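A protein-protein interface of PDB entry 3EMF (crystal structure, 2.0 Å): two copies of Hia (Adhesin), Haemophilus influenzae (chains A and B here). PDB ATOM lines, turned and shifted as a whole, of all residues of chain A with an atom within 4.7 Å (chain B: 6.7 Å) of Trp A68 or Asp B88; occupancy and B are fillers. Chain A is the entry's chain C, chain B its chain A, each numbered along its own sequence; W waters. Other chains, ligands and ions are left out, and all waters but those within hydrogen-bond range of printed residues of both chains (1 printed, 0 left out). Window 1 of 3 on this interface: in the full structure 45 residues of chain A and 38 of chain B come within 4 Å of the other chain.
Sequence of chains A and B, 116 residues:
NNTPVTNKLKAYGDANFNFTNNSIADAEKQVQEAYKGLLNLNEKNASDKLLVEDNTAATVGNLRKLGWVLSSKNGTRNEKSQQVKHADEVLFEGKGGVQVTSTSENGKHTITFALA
The backbone NH (N) of Ala B87 is in hydrogen-bond range of the backbone carbonyl oxygen (O) of Gly A67. The backbone carbonyl oxygen of Asp B88 lies within hydrogen-bond range of the backbone NH of Val A69, 2.9 Å away. The backbone NH (N) of Val B90 is in hydrogen-bond range of the backbone carbonyl oxygen (O) of Val A69 (2.8 Å). The side-chain hydroxyl (OH) of Tyr A35 lies close to the backbone carbonyl oxygen (O) of Ala B87, 3.4 Å away.
Among the printed residues, merely in contact across the chains: Gly A67 with His B86, Val A69 with Glu B89, Tyr A35 with Glu B89, Leu A70 with Phe B92, Trp A68 with Asp B88, Leu A70 with Val B90, Trp A68 with Trp B68, Tyr A35 with Asp B88 and Trp A68 with Val B90.
Trp A68 touches its own counterpart, Trp B68. Trp A68 touches Val B90, but with the chains exchanged Val A90 does not touch Trp B68 (7.5 Å). Of the 13 pairs that touch across the chains among the printed residues, 1 has its exchanged pair printed and touching as well.
The backbone carbonyl oxygen of Leu A70 sits at hydrogen-bond distance from the backbone NH of Gln A82 (2.8 Å). O of Trp B68 sits at hydrogen-bond distance from N of Val B84 (2.8 Å). The backbone NH (N) of Val A84 sits at hydrogen-bond distance from the backbone carbonyl oxygen (O) of Trp A68. The backbone NH of Lys B85 sits at hydrogen-bond distance from the side-chain carboxylate of Asp B88, at 2.9 Å.
Trp A68 touches just these residues of chain B: Trp B68, Asp B88 and Val B90. Of the printed residues of chain B, Leu A70 touches Val B90 and Phe B92. Of the printed residues of chain A, Trp B68 touches Trp A68. Gln B83 touches none of the printed residues of chain A. Of the printed residues of chain A, Ala B87 touches Tyr A35 (3.2 Å) and Gly A67 (2.7 Å). Of the printed residues of chain A, Glu B89 touches Tyr A35 (3.3 Å) and Val A69 (3.2 Å). Printed residues of chain A within 4 Å of Val B90: Trp A68 (3.97 Å), Val A69 (2.8 Å) and Leu A70 (3.5 Å). The nearest residue of chain B that does not touch Trp A68 is Val B84 (4.1 Å). The nearest printed residue of chain A that does not touch Asp B88 is Gly A67 (4.7 Å).
Printed residues of chain A that touch a printed residue of chain B: Tyr A35, Gly A67, Trp A68, Val A69 and Leu A70. Along chain A the printed residues that touch a printed residue of chain B span positions 35 to 70. Printed residues of chain B that touch a printed residue of chain A: Trp B68, His B86, Ala B87, Asp B88, Glu B89, Val B90 and Phe B92. Among the printed residues, 13 pairs touch across the chains. Among the printed residues, no Asp or Glu carboxylate lies within 4 Å of a Lys or Arg side-chain nitrogen of the other chain.
Water W1 lies within hydrogen-bond range of the side-chain hydroxyl of Tyr A35 (2.6 Å) and the backbone carbonyl oxygen of Ala B87 (3.5 Å).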
ATOM      1  N   TYR A  35       9.235 -14.881  20.931  1.00  0.00           N
ATOM      2  CA  TYR A  35       9.668 -13.796  20.041  1.00  0.00           C
ATOM      3  C   TYR A  35      10.473 -14.286  18.838  1.00  0.00           C
ATOM      4  O   TYR A  35      10.646 -13.556  17.867  1.00  0.00           O
ATOM      5  CB  TYR A  35      10.450 -12.725  20.815  1.00  0.00           C
ATOM      6  CG  TYR A  35       9.577 -11.755  21.570  1.00  0.00           C
ATOM      7  CD1 TYR A  35       9.032 -10.655  20.930  1.00  0.00           C
ATOM      8  CD2 TYR A  35       9.310 -11.928  22.934  1.00  0.00           C
ATOM      9  CE1 TYR A  35       8.234  -9.756  21.611  1.00  0.00           C
ATOM     10  CE2 TYR A  35       8.507 -11.024  23.620  1.00  0.00           C
ATOM     11  CZ  TYR A  35       7.980  -9.943  22.947  1.00  0.00           C
ATOM     12  OH  TYR A  35       7.184  -9.033  23.593  1.00  0.00           O
ATOM     13  N   LEU A  38      10.114 -13.484  14.916  1.00  0.00           N
ATOM     14  CA  LEU A  38       9.468 -12.189  14.723  1.00  0.00           C
ATOM     15  C   LEU A  38      10.492 -11.167  14.252  1.00  0.00           C
ATOM     16  O   LEU A  38      11.661 -11.207  14.647  1.00  0.00           O
ATOM     17  CB  LEU A  38       8.772 -11.706  15.994  1.00  0.00           C
ATOM     18  CG  LEU A  38       7.526 -12.478  16.447  1.00  0.00           C
ATOM     19  CD1 LEU A  38       6.815 -11.716  17.568  1.00  0.00           C
ATOM     20  CD2 LEU A  38       6.573 -12.718  15.263  1.00  0.00           C
ATOM     21  N   GLY A  67       4.200  -9.725  13.785  1.00  0.00           N
ATOM     22  CA  GLY A  67       3.293 -10.271  14.763  1.00  0.00           C
ATOM     23  C   GLY A  67       3.456  -9.647  16.134  1.00  0.00           C
ATOM     24  O   GLY A  67       4.130  -8.624  16.292  1.00  0.00           O
ATOM     25  N   TRP A  68       2.816 -10.269  17.122  1.00  0.00           N
ATOM     26  CA  TRP A  68       2.884  -9.820  18.513  1.00  0.00           C
ATOM     27  C   TRP A  68       2.828 -11.033  19.445  1.00  0.00           C
ATOM     28  O   TRP A  68       2.553 -12.157  19.007  1.00  0.00           O
ATOM     29  CB  TRP A  68       1.762  -8.811  18.821  1.00  0.00           C
ATOM     30  CG  TRP A  68       0.370  -9.300  18.463  1.00  0.00           C
ATOM     31  CD1 TRP A  68      -0.206  -9.304  17.215  1.00  0.00           C
ATOM     32  CD2 TRP A  68      -0.616  -9.824  19.355  1.00  0.00           C
ATOM     33  NE1 TRP A  68      -1.475  -9.826  17.278  1.00  0.00           N
ATOM     34  CE2 TRP A  68      -1.760 -10.143  18.577  1.00  0.00           C
ATOM     35  CE3 TRP A  68      -0.644 -10.077  20.732  1.00  0.00           C
ATOM     36  CZ2 TRP A  68      -2.914 -10.694  19.128  1.00  0.00           C
ATOM     37  CZ3 TRP A  68      -1.804 -10.623  21.287  1.00  0.00           C
ATOM     38  CH2 TRP A  68      -2.925 -10.926  20.482  1.00  0.00           C
ATOM     39  N   VAL A  69       3.107 -10.816  20.724  1.00  0.00           N
ATOM     40  CA  VAL A  69       3.147 -11.925  21.671  1.00  0.00           C
ATOM     41  C   VAL A  69       1.962 -11.850  22.607  1.00  0.00           C
ATOM     42  O   VAL A  69       1.650 -10.798  23.144  1.00  0.00           O
ATOM     43  CB  VAL A  69       4.490 -11.985  22.439  1.00  0.00           C
ATOM     44  CG1 VAL A  69       4.463 -13.092  23.491  1.00  0.00           C
ATOM     45  CG2 VAL A  69       5.612 -12.245  21.451  1.00  0.00           C
ATOM     46  N   LEU A  70       1.294 -12.992  22.734  1.00  0.00           N
ATOM     47  CA  LEU A  70       0.138 -13.179  23.568  1.00  0.00           C
ATOM     48  C   LEU A  70       0.557 -14.011  24.777  1.00  0.00           C
ATOM     49  O   LEU A  70       1.076 -15.133  24.641  1.00  0.00           O
ATOM     50  CB  LEU A  70      -0.935 -13.939  22.772  1.00  0.00           C
ATOM     51  CG  LEU A  70      -2.200 -14.361  23.506  1.00  0.00           C
ATOM     52  CD1 LEU A  70      -2.989 -13.129  23.970  1.00  0.00           C
ATOM     53  CD2 LEU A  70      -3.034 -15.280  22.596  1.00  0.00           C
ATOM     54  N   GLN A  82       2.946 -17.034  23.680  1.00  0.00           N
ATOM     55  CA  GLN A  82       2.929 -17.617  22.348  1.00  0.00           C
ATOM     56  C   GLN A  82       2.929 -16.515  21.316  1.00  0.00           C
ATOM     57  O   GLN A  82       2.570 -15.391  21.598  1.00  0.00           O
ATOM     58  CB  GLN A  82       1.730 -18.554  22.134  1.00  0.00           C
ATOM     59  CG  GLN A  82       0.412 -18.020  22.645  1.00  0.00           C
ATOM     60  CD  GLN A  82       0.107 -18.527  24.031  1.00  0.00           C
ATOM     61  OE1 GLN A  82       0.004 -17.755  24.991  1.00  0.00           O
ATOM     62  NE2 GLN A  82      -0.015 -19.842  24.153  1.00  0.00           N
ATOM     63  N   GLN A  83       3.311 -16.879  20.107  1.00  0.00           N
ATOM     64  CA  GLN A  83       3.530 -15.946  19.031  1.00  0.00           C
ATOM     65  C   GLN A  83       2.261 -15.819  18.198  1.00  0.00           C
ATOM     66  O   GLN A  83       1.702 -16.825  17.783  1.00  0.00           O
ATOM     67  CB  GLN A  83       4.637 -16.528  18.167  1.00  0.00           C
ATOM     68  CG  GLN A  83       5.136 -15.633  17.096  1.00  0.00           C
ATOM     69  CD  GLN A  83       6.382 -16.188  16.482  1.00  0.00           C
ATOM     70  OE1 GLN A  83       6.326 -16.856  15.461  1.00  0.00           O
ATOM     71  NE2 GLN A  83       7.520 -15.934  17.115  1.00  0.00           N
ATOM     72  N   VAL A  84       1.796 -14.594  17.975  1.00  0.00           N
ATOM     73  CA  VAL A  84       0.659 -14.367  17.095  1.00  0.00           C
ATOM     74  C   VAL A  84       1.119 -13.683  15.802  1.00  0.00           C
ATOM     75  O   VAL A  84       1.465 -12.505  15.815  1.00  0.00           O
ATOM     76  CB  VAL A  84      -0.433 -13.502  17.749  1.00  0.00           C
ATOM     77  CG1 VAL A  84      -1.674 -13.402  16.809  1.00  0.00           C
ATOM     78  CG2 VAL A  84      -0.818 -14.059  19.101  1.00  0.00           C
ATOM     79  N   VAL A  90      -7.000 -16.023  17.573  1.00  0.00           N
ATOM     80  CA  VAL A  90      -6.957 -15.995  19.031  1.00  0.00           C
ATOM     81  C   VAL A  90      -8.372 -16.108  19.546  1.00  0.00           C
ATOM     82  O   VAL A  90      -9.202 -15.253  19.288  1.00  0.00           O
ATOM     83  CB  VAL A  90      -6.336 -14.686  19.589  1.00  0.00           C
ATOM     84  CG1 VAL A  90      -6.295 -14.735  21.114  1.00  0.00           C
ATOM     85  CG2 VAL A  90      -4.940 -14.470  19.029  1.00  0.00           C
ATOM     86  N   TRP B  68      -2.615  -2.399  16.201  1.00  0.00           N
ATOM     87  CA  TRP B  68      -4.030  -2.328  16.500  1.00  0.00           C
ATOM     88  C   TRP B  68      -4.172  -1.735  17.894  1.00  0.00           C
ATOM     89  O   TRP B  68      -3.209  -1.707  18.668  1.00  0.00           O
ATOM     90  CB  TRP B  68      -4.690  -3.725  16.398  1.00  0.00           C
ATOM     91  CG  TRP B  68      -3.987  -4.822  17.128  1.00  0.00           C
ATOM     92  CD1 TRP B  68      -2.884  -5.534  16.703  1.00  0.00           C
ATOM     93  CD2 TRP B  68      -4.352  -5.373  18.401  1.00  0.00           C
ATOM     94  NE1 TRP B  68      -2.554  -6.478  17.645  1.00  0.00           N
ATOM     95  CE2 TRP B  68      -3.446  -6.407  18.686  1.00  0.00           C
ATOM     96  CE3 TRP B  68      -5.370  -5.099  19.322  1.00  0.00           C
ATOM     97  CZ2 TRP B  68      -3.513  -7.155  19.867  1.00  0.00           C
ATOM     98  CZ3 TRP B  68      -5.434  -5.843  20.487  1.00  0.00           C
ATOM     99  CH2 TRP B  68      -4.519  -6.860  20.745  1.00  0.00           C
ATOM    100  N   GLN B  83      -1.523   1.029  22.204  1.00  0.00           N
ATOM    101  CA  GLN B  83      -1.280   0.497  20.877  1.00  0.00           C
ATOM    102  C   GLN B  83      -0.479  -0.758  20.959  1.00  0.00           C
ATOM    103  O   GLN B  83       0.570  -0.787  21.591  1.00  0.00           O
ATOM    104  CB  GLN B  83      -0.495   1.479  20.025  1.00  0.00           C
ATOM    105  CG  GLN B  83      -1.119   2.803  19.939  1.00  0.00           C
ATOM    106  CD  GLN B  83      -0.336   3.748  19.069  1.00  0.00           C
ATOM    107  OE1 GLN B  83       0.843   3.533  18.783  1.00  0.00           O
ATOM    108  NE2 GLN B  83      -0.997   4.814  18.636  1.00  0.00           N
ATOM    109  N   VAL B  84      -0.961  -1.797  20.288  1.00  0.00           N
ATOM    110  CA  VAL B  84      -0.190  -3.005  20.139  1.00  0.00           C
ATOM    111  C   VAL B  84       0.492  -2.959  18.787  1.00  0.00           C
ATOM    112  O   VAL B  84      -0.146  -3.138  17.747  1.00  0.00           O
ATOM    113  CB  VAL B  84      -1.079  -4.229  20.232  1.00  0.00           C
ATOM    114  CG1 VAL B  84      -0.227  -5.500  20.145  1.00  0.00           C
ATOM    115  CG2 VAL B  84      -1.839  -4.168  21.531  1.00  0.00           C
ATOM    116  N   LYS B  85       1.792  -2.703  18.802  1.00  0.00           N
ATOM    117  CA  LYS B  85       2.544  -2.611  17.567  1.00  0.00           C
ATOM    118  C   LYS B  85       3.295  -3.895  17.324  1.00  0.00           C
ATOM    119  O   LYS B  85       3.203  -4.831  18.123  1.00  0.00           O
ATOM    120  CB  LYS B  85       3.463  -1.386  17.598  1.00  0.00           C
ATOM    121  CG  LYS B  85       2.643  -0.088  17.636  1.00  0.00           C
ATOM    122  CD  LYS B  85       3.064   0.906  16.563  1.00  0.00           C
ATOM    123  CE  LYS B  85       4.389   1.552  16.896  1.00  0.00           C
ATOM    124  NZ  LYS B  85       4.650   2.742  16.033  1.00  0.00           N
ATOM    125  N   HIS B  86       4.035  -3.968  16.221  1.00  0.00           N
ATOM    126  CA  HIS B  86       4.751  -5.196  15.964  1.00  0.00           C
ATOM    127  C   HIS B  86       5.679  -5.493  17.131  1.00  0.00           C
ATOM    128  O   HIS B  86       6.374  -4.588  17.630  1.00  0.00           O
ATOM    129  CB  HIS B  86       5.581  -5.110  14.699  1.00  0.00           C
ATOM    130  CG  HIS B  86       6.506  -6.273  14.535  1.00  0.00           C
ATOM    131  ND1 HIS B  86       7.848  -6.210  14.834  1.00  0.00           N
ATOM    132  CD2 HIS B  86       6.260  -7.552  14.174  1.00  0.00           C
ATOM    133  CE1 HIS B  86       8.394  -7.401  14.651  1.00  0.00           C
ATOM    134  NE2 HIS B  86       7.452  -8.230  14.235  1.00  0.00           N
ATOM    135  N   ALA B  87       5.689  -6.759  17.549  1.00  0.00           N
ATOM    136  CA  ALA B  87       6.593  -7.257  18.590  1.00  0.00           C
ATOM    137  C   ALA B  87       6.276  -6.743  19.983  1.00  0.00           C
ATOM    138  O   ALA B  87       7.063  -6.914  20.914  1.00  0.00           O
ATOM    139  CB  ALA B  87       8.076  -7.001  18.227  1.00  0.00           C
ATOM    140  N   ASP B  88       5.117  -6.127  20.133  1.00  0.00           N
ATOM    141  CA  ASP B  88       4.606  -5.850  21.464  1.00  0.00           C
ATOM    142  C   ASP B  88       4.044  -7.122  22.105  1.00  0.00           C
ATOM    143  O   ASP B  88       3.895  -8.158  21.450  1.00  0.00           O
ATOM    144  CB  ASP B  88       3.540  -4.769  21.412  1.00  0.00           C
ATOM    145  CG  ASP B  88       4.137  -3.348  21.236  1.00  0.00           C
ATOM    146  OD1 ASP B  88       5.384  -3.204  21.153  1.00  0.00           O
ATOM    147  OD2 ASP B  88       3.345  -2.382  21.179  1.00  0.00           O
ATOM    148  N   GLU B  89       3.760  -7.038  23.400  1.00  0.00           N
ATOM    149  CA  GLU B  89       3.241  -8.174  24.144  1.00  0.00           C
ATOM    150  C   GLU B  89       1.969  -7.784  24.873  1.00  0.00           C
ATOM    151  O   GLU B  89       1.879  -6.701  25.458  1.00  0.00           O
ATOM    152  CB  GLU B  89       4.288  -8.724  25.115  1.00  0.00           C
ATOM    153  CG  GLU B  89       3.786  -9.886  25.990  1.00  0.00           C
ATOM    154  CD  GLU B  89       4.890 -10.477  26.874  1.00  0.00           C
ATOM    155  OE1 GLU B  89       5.970  -9.848  26.986  1.00  0.00           O
ATOM    156  OE2 GLU B  89       4.682 -11.569  27.458  1.00  0.00           O
ATOM    157  N   VAL B  90       0.969  -8.652  24.779  1.00  0.00           N
ATOM    158  CA  VAL B  90      -0.274  -8.478  25.508  1.00  0.00           C
ATOM    159  C   VAL B  90      -0.406  -9.633  26.480  1.00  0.00           C
ATOM    160  O   VAL B  90      -0.436 -10.805  26.089  1.00  0.00           O
ATOM    161  CB  VAL B  90      -1.506  -8.417  24.579  1.00  0.00           C
ATOM    162  CG1 VAL B  90      -2.764  -8.245  25.397  1.00  0.00           C
ATOM    163  CG2 VAL B  90      -1.360  -7.285  23.593  1.00  0.00           C
ATOM    164  N   PHE B  92      -2.644 -11.276  29.444  1.00  0.00           N
ATOM    165  CA  PHE B  92      -3.922 -11.378  30.121  1.00  0.00           C
ATOM    166  C   PHE B  92      -3.647 -12.079  31.442  1.00  0.00           C
ATOM    167  O   PHE B  92      -3.175 -13.215  31.463  1.00  0.00           O
ATOM    168  CB  PHE B  92      -4.933 -12.159  29.254  1.00  0.00           C
ATOM    169  CG  PHE B  92      -5.260 -11.458  27.973  1.00  0.00           C
ATOM    170  CD1 PHE B  92      -6.340 -10.596  27.900  1.00  0.00           C
ATOM    171  CD2 PHE B  92      -4.439 -11.597  26.861  1.00  0.00           C
ATOM    172  CE1 PHE B  92      -6.625  -9.926  26.732  1.00  0.00           C
ATOM    173  CE2 PHE B  92      -4.719 -10.913  25.684  1.00  0.00           C
ATOM    174  CZ  PHE B  92      -5.811 -10.084  25.622  1.00  0.00           C
HETATM  175  O   HOH W   1       7.121  -6.540  24.384  1.00  0.00           O
